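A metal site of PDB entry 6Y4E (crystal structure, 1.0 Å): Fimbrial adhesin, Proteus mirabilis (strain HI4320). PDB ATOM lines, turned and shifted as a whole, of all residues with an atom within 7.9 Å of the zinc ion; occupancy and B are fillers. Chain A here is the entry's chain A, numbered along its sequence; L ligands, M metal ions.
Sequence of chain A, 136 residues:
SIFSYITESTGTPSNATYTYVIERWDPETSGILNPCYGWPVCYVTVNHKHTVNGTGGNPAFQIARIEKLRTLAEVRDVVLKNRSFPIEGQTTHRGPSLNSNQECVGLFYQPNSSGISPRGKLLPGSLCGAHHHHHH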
ATOM      1  N   PRO A  13      22.728  -9.719 -24.858  1.00  0.00           N
ATOM      2  CA  PRO A  13      21.268  -9.819 -24.960  1.00  0.00           C
ATOM      3  C   PRO A  13      20.512  -8.900 -24.032  1.00  0.00           C
ATOM      4  O   PRO A  13      19.381  -8.520 -24.364  1.00  0.00           O
ATOM      5  CB  PRO A  13      20.994 -11.295 -24.631  1.00  0.00           C
ATOM      6  CG  PRO A  13      22.244 -11.983 -25.120  1.00  0.00           C
ATOM      7  CD  PRO A  13      23.372 -11.049 -24.789  1.00  0.00           C
ATOM      8  N   SER A  14      21.101  -8.562 -22.878  1.00  0.00           N
ATOM      9  CA  SER A  14      20.444  -7.712 -21.900  1.00  0.00           C
ATOM     10  C   SER A  14      20.938  -6.269 -21.927  1.00  0.00           C
ATOM     11  O   SER A  14      20.470  -5.455 -21.138  1.00  0.00           O
ATOM     12  CB  SER A  14      20.639  -8.283 -20.507  1.00  0.00           C
ATOM     13  OG  SER A  14      22.008  -8.391 -20.258  1.00  0.00           O
ATOM     14  N   ALA A  16      21.980  -4.084 -25.198  1.00  0.00           N
ATOM     15  CA  ALA A  16      22.162  -4.174 -26.623  1.00  0.00           C
ATOM     16  C   ALA A  16      21.820  -2.849 -27.280  1.00  0.00           C
ATOM     17  O   ALA A  16      20.933  -2.121 -26.841  1.00  0.00           O
ATOM     18  CB  ALA A  16      21.254  -5.251 -27.232  1.00  0.00           C
ATOM     19  N   TYR A  18      20.534  -1.509 -30.942  1.00  0.00           N
ATOM     20  CA  TYR A  18      19.939  -1.933 -32.185  1.00  0.00           C
ATOM     21  C   TYR A  18      20.027  -0.811 -33.204  1.00  0.00           C
ATOM     22  O   TYR A  18      19.611   0.329 -32.920  1.00  0.00           O
ATOM     23  CB  TYR A  18      18.451  -2.234 -32.009  1.00  0.00           C
ATOM     24  CG  TYR A  18      18.087  -3.143 -30.876  1.00  0.00           C
ATOM     25  CD1 TYR A  18      18.805  -4.299 -30.581  1.00  0.00           C
ATOM     26  CD2 TYR A  18      16.972  -2.870 -30.104  1.00  0.00           C
ATOM     27  CE1 TYR A  18      18.416  -5.134 -29.549  1.00  0.00           C
ATOM     28  CE2 TYR A  18      16.584  -3.696 -29.094  1.00  0.00           C
ATOM     29  CZ  TYR A  18      17.295  -4.823 -28.806  1.00  0.00           C
ATOM     30  OH  TYR A  18      16.817  -5.627 -27.781  1.00  0.00           O
ATOM     31  N   ASN A  47       9.475   1.956 -30.781  1.00  0.00           N
ATOM     32  CA  ASN A  47       9.888   1.310 -29.546  1.00  0.00           C
ATOM     33  C   ASN A  47      10.402  -0.076 -29.894  1.00  0.00           C
ATOM     34  O   ASN A  47      10.331  -0.504 -31.045  1.00  0.00           O
ATOM     35  CB  ASN A  47       8.697   1.259 -28.550  1.00  0.00           C
ATOM     36  CG  ASN A  47       9.106   1.181 -27.085  1.00  0.00           C
ATOM     37  OD1 ASN A  47      10.246   0.853 -26.729  1.00  0.00           O
ATOM     38  ND2 ASN A  47       8.151   1.448 -26.209  1.00  0.00           N
ATOM     39  N   HIS A  48      10.941  -0.751 -28.897  1.00  0.00           N
ATOM     40  CA  HIS A  48      11.418  -2.114 -29.059  1.00  0.00           C
ATOM     41  C   HIS A  48      10.708  -3.047 -28.087  1.00  0.00           C
ATOM     42  O   HIS A  48      10.211  -2.646 -27.029  1.00  0.00           O
ATOM     43  CB  HIS A  48      12.950  -2.197 -28.834  1.00  0.00           C
ATOM     44  CG  HIS A  48      13.373  -1.881 -27.449  1.00  0.00           C
ATOM     45  ND1 HIS A  48      13.482  -0.598 -26.979  1.00  0.00           N
ATOM     46  CD2 HIS A  48      13.642  -2.697 -26.399  1.00  0.00           C
ATOM     47  CE1 HIS A  48      13.812  -0.638 -25.701  1.00  0.00           C
ATOM     48  NE2 HIS A  48      13.916  -1.888 -25.335  1.00  0.00           N
ATOM     49  N   LYS A  49      10.696  -4.334 -28.444  1.00  0.00           N
ATOM     50  CA  LYS A  49      10.279  -5.377 -27.516  1.00  0.00           C
ATOM     51  C   LYS A  49      11.298  -5.450 -26.394  1.00  0.00           C
ATOM     52  O   LYS A  49      12.481  -5.698 -26.621  1.00  0.00           O
ATOM     53  CB  LYS A  49      10.161  -6.716 -28.229  1.00  0.00           C
ATOM     54  CG  LYS A  49       9.019  -6.811 -29.211  1.00  0.00           C
ATOM     55  CD  LYS A  49       8.911  -8.182 -29.801  1.00  0.00           C
ATOM     56  CE  LYS A  49       7.850  -8.275 -30.864  1.00  0.00           C
ATOM     57  NZ  LYS A  49       7.758  -9.634 -31.422  1.00  0.00           N
ATOM     58  N   HIS A  50      10.833  -5.218 -25.166  1.00  0.00           N
ATOM     59  CA  HIS A  50      11.710  -5.095 -24.003  1.00  0.00           C
ATOM     60  C   HIS A  50      11.682  -6.338 -23.124  1.00  0.00           C
ATOM     61  O   HIS A  50      12.597  -6.531 -22.319  1.00  0.00           O
ATOM     62  CB  HIS A  50      11.194  -3.888 -23.203  1.00  0.00           C
ATOM     63  CG  HIS A  50      11.963  -3.579 -21.978  1.00  0.00           C
ATOM     64  ND1 HIS A  50      13.221  -3.063 -22.002  1.00  0.00           N
ATOM     65  CD2 HIS A  50      11.600  -3.695 -20.675  1.00  0.00           C
ATOM     66  CE1 HIS A  50      13.628  -2.875 -20.744  1.00  0.00           C
ATOM     67  NE2 HIS A  50      12.671  -3.253 -19.923  1.00  0.00           N
ATOM     68  N   THR A  51      10.642  -7.128 -23.231  1.00  0.00           N
ATOM     69  CA  THR A  51      10.426  -8.291 -22.409  1.00  0.00           C
ATOM     70  C   THR A  51      10.168  -9.470 -23.307  1.00  0.00           C
ATOM     71  O   THR A  51       9.884  -9.336 -24.509  1.00  0.00           O
ATOM     72  CB  THR A  51       9.207  -8.126 -21.491  1.00  0.00           C
ATOM     73  OG1 THR A  51       8.006  -8.097 -22.274  1.00  0.00           O
ATOM     74  CG2 THR A  51       9.319  -6.887 -20.623  1.00  0.00           C
ATOM     75  N   THR A  55       6.337  -6.702 -24.784  1.00  0.00           N
ATOM     76  CA  THR A  55       5.889  -5.392 -24.369  1.00  0.00           C
ATOM     77  C   THR A  55       7.013  -4.385 -24.578  1.00  0.00           C
ATOM     78  O   THR A  55       8.152  -4.745 -24.845  1.00  0.00           O
ATOM     79  CB  THR A  55       5.421  -5.436 -22.924  1.00  0.00           C
ATOM     80  OG1 THR A  55       6.500  -5.809 -22.057  1.00  0.00           O
ATOM     81  CG2 THR A  55       4.308  -6.467 -22.754  1.00  0.00           C
ATOM     82  N   GLY A  56       6.679  -3.100 -24.501  1.00  0.00           N
ATOM     83  CA  GLY A  56       7.592  -2.063 -24.926  1.00  0.00           C
ATOM     84  C   GLY A  56       8.601  -1.601 -23.887  1.00  0.00           C
ATOM     85  O   GLY A  56       8.371  -1.635 -22.676  1.00  0.00           O
ATOM     86  N   GLY A  57       9.716  -1.124 -24.383  1.00  0.00           N
ATOM     87  CA  GLY A  57      10.715  -0.466 -23.573  1.00  0.00           C
ATOM     88  C   GLY A  57      10.504   1.026 -23.499  1.00  0.00           C
ATOM     89  O   GLY A  57       9.394   1.519 -23.630  1.00  0.00           O
ATOM     90  N   ASN A  58      11.585   1.744 -23.259  1.00  0.00           N
ATOM     91  CA  ASN A  58      11.608   3.190 -23.371  1.00  0.00           C
ATOM     92  C   ASN A  58      11.653   3.550 -24.852  1.00  0.00           C
ATOM     93  O   ASN A  58      12.595   3.135 -25.539  1.00  0.00           O
ATOM     94  CB  ASN A  58      12.818   3.767 -22.665  1.00  0.00           C
ATOM     95  CG  ASN A  58      12.802   5.273 -22.630  1.00  0.00           C
ATOM     96  OD1 ASN A  58      11.752   5.897 -22.588  1.00  0.00           O
ATOM     97  ND2 ASN A  58      13.976   5.877 -22.710  1.00  0.00           N
ATOM     98  N   THR A  91      18.631   2.474 -31.119  1.00  0.00           N
ATOM     99  CA  THR A  91      18.024   2.515 -29.796  1.00  0.00           C
ATOM    100  C   THR A  91      18.659   1.417 -28.953  1.00  0.00           C
ATOM    101  O   THR A  91      19.180   0.441 -29.467  1.00  0.00           O
ATOM    102  CB  THR A  91      16.496   2.426 -29.902  1.00  0.00           C
ATOM    103  OG1 THR A  91      15.903   2.802 -28.654  1.00  0.00           O
ATOM    104  CG2 THR A  91      15.999   1.048 -30.252  1.00  0.00           C
ATOM    105  N   THR A  92      18.640   1.577 -27.636  1.00  0.00           N
ATOM    106  CA  THR A  92      19.379   0.670 -26.760  1.00  0.00           C
ATOM    107  C   THR A  92      18.456   0.014 -25.748  1.00  0.00           C
ATOM    108  O   THR A  92      17.692   0.687 -25.060  1.00  0.00           O
ATOM    109  CB  THR A  92      20.550   1.368 -26.052  1.00  0.00           C
ATOM    110  OG1 THR A  92      21.520   1.837 -27.000  1.00  0.00           O
ATOM    111  CG2 THR A  92      21.258   0.431 -25.041  1.00  0.00           C
ATOM    112  N   HIS A  93      18.564  -1.303 -25.629  1.00  0.00           N
ATOM    113  CA  HIS A  93      17.819  -2.128 -24.697  1.00  0.00           C
ATOM    114  C   HIS A  93      18.715  -2.497 -23.531  1.00  0.00           C
ATOM    115  O   HIS A  93      19.801  -3.051 -23.720  1.00  0.00           O
ATOM    116  CB  HIS A  93      17.342  -3.389 -25.391  1.00  0.00           C
ATOM    117  CG  HIS A  93      16.804  -4.398 -24.454  1.00  0.00           C
ATOM    118  ND1 HIS A  93      15.636  -4.207 -23.729  1.00  0.00           N
ATOM    119  CD2 HIS A  93      17.277  -5.607 -24.111  1.00  0.00           C
ATOM    120  CE1 HIS A  93      15.431  -5.276 -22.989  1.00  0.00           C
ATOM    121  NE2 HIS A  93      16.420  -6.141 -23.197  1.00  0.00           N
ATOM    122  N   ARG A  94      18.256  -2.176 -22.317  1.00  0.00           N
ATOM    123  CA  ARG A  94      18.897  -2.605 -21.085  1.00  0.00           C
ATOM    124  C   ARG A  94      17.783  -3.199 -20.244  1.00  0.00           C
ATOM    125  O   ARG A  94      16.892  -2.472 -19.818  1.00  0.00           O
ATOM    126  CB  ARG A  94      19.537  -1.416 -20.372  1.00  0.00           C
ATOM    127  CG  ARG A  94      20.666  -0.779 -21.161  1.00  0.00           C
ATOM    128  CD  ARG A  94      21.154   0.525 -20.568  1.00  0.00           C
ATOM    129  NE  ARG A  94      22.234   1.103 -21.369  1.00  0.00           N
ATOM    130  CZ  ARG A  94      22.116   2.142 -22.188  1.00  0.00           C
ATOM    131  NH1 ARG A  94      20.956   2.775 -22.337  1.00  0.00           N
ATOM    132  NH2 ARG A  94      23.182   2.568 -22.859  1.00  0.00           N
ATOM    133  N   GLY A  95      17.811  -4.499 -20.045  1.00  0.00           N
ATOM    134  CA  GLY A  95      16.699  -5.157 -19.406  1.00  0.00           C
ATOM    135  C   GLY A  95      16.806  -6.663 -19.562  1.00  0.00           C
ATOM    136  O   GLY A  95      17.904  -7.220 -19.628  1.00  0.00           O
ATOM    137  N   PRO A  96      15.663  -7.329 -19.633  1.00  0.00           N
ATOM    138  CA  PRO A  96      15.661  -8.785 -19.821  1.00  0.00           C
ATOM    139  C   PRO A  96      16.531  -9.231 -20.985  1.00  0.00           C
ATOM    140  O   PRO A  96      16.621  -8.580 -22.013  1.00  0.00           O
ATOM    141  CB  PRO A  96      14.194  -9.088 -20.106  1.00  0.00           C
ATOM    142  CG  PRO A  96      13.474  -8.068 -19.305  1.00  0.00           C
ATOM    143  CD  PRO A  96      14.302  -6.820 -19.448  1.00  0.00           C
ATOM    144  N   LEU A  98      17.279 -10.951 -24.269  1.00  0.00           N
ATOM    145  CA  LEU A  98      16.485 -11.277 -25.449  1.00  0.00           C
ATOM    146  C   LEU A  98      17.374 -11.887 -26.520  1.00  0.00           C
ATOM    147  O   LEU A  98      18.450 -11.354 -26.789  1.00  0.00           O
ATOM    148  CB  LEU A  98      15.820 -10.031 -26.043  1.00  0.00           C
ATOM    149  CG  LEU A  98      14.965  -9.247 -25.058  1.00  0.00           C
ATOM    150  CD1 LEU A  98      14.485  -7.951 -25.735  1.00  0.00           C
ATOM    151  CD2 LEU A  98      13.784 -10.054 -24.574  1.00  0.00           C
ATOM    152  N   ILE A 116       9.697   2.955 -19.515  1.00  0.00           N
ATOM    153  CA  ILE A 116       9.372   1.577 -19.824  1.00  0.00           C
ATOM    154  C   ILE A 116       7.869   1.479 -20.054  1.00  0.00           C
ATOM    155  O   ILE A 116       7.078   2.179 -19.418  1.00  0.00           O
ATOM    156  CB  ILE A 116       9.869   0.620 -18.725  1.00  0.00           C
ATOM    157  CG1 ILE A 116      11.365   0.791 -18.447  1.00  0.00           C
ATOM    158  CG2 ILE A 116       9.563  -0.811 -19.065  1.00  0.00           C
ATOM    159  CD1 ILE A 116      12.218   0.534 -19.648  1.00  0.00           C
HETATM  160  O1  LIG L   1      15.608  -1.173 -22.596  1.00  0.00           O
HETATM  161  O2  LIG L   1      13.912   0.222 -22.742  1.00  0.00           O
HETATM  162  C1  LIG L   1      15.099  -0.038 -22.411  1.00  0.00           C
HETATM  163  C2  LIG L   1      16.028   1.051 -21.918  1.00  0.00           C
HETATM  164  O3  LIG L   1      17.381   0.739 -22.158  1.00  0.00           O
HETATM  165  C3  LIG L   1      15.807   1.206 -20.428  1.00  0.00           C
HETATM  166  O4  LIG L   1      15.770  -0.069 -19.875  1.00  0.00           O
HETATM  167  C4  LIG L   1      16.949   2.008 -19.813  1.00  0.00           C
HETATM  168  O5  LIG L   1      17.665   1.514 -18.913  1.00  0.00           O
HETATM  169  O6  LIG L   1      17.146   3.180 -20.220  1.00  0.00           O
HETATM  170 ZN    ZN M   1      14.479  -2.536 -23.495  1.00  0.00          ZN
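Arg 94 touches the zinc ion.
Of the 21 residues printed, 4 come within 4 Å of the zinc ion.
The nearest printed residue that does not touch the zinc ion is Gly 57 (4.3 Å).
The zinc ion is bound by an oxygen (O1) of the ligand, a ring nitrogen (ND1) of His 50, a ring nitrogen (NE2) of His 48 and a ring nitrogen (ND1) of His 93.
The zinc ion has four donor atoms within binding distance.
The backbone carbonyl oxygen of Pro 96 sits at hydrogen-bond distance from a ring nitrogen (NE2) of His 93, 2.7 Å away.
The backbone NH of His 93 sits at hydrogen-bond distance from the backbone carbonyl oxygen of Ala 16 (2.8 Å).
The backbone carbonyl oxygen (O) of His 48 sits at hydrogen-bond distance from the backbone NH (N) of Gly 57 (3.1 Å).
N of His 50 is in hydrogen-bond range of O of Thr 55, at 2.7 Å.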
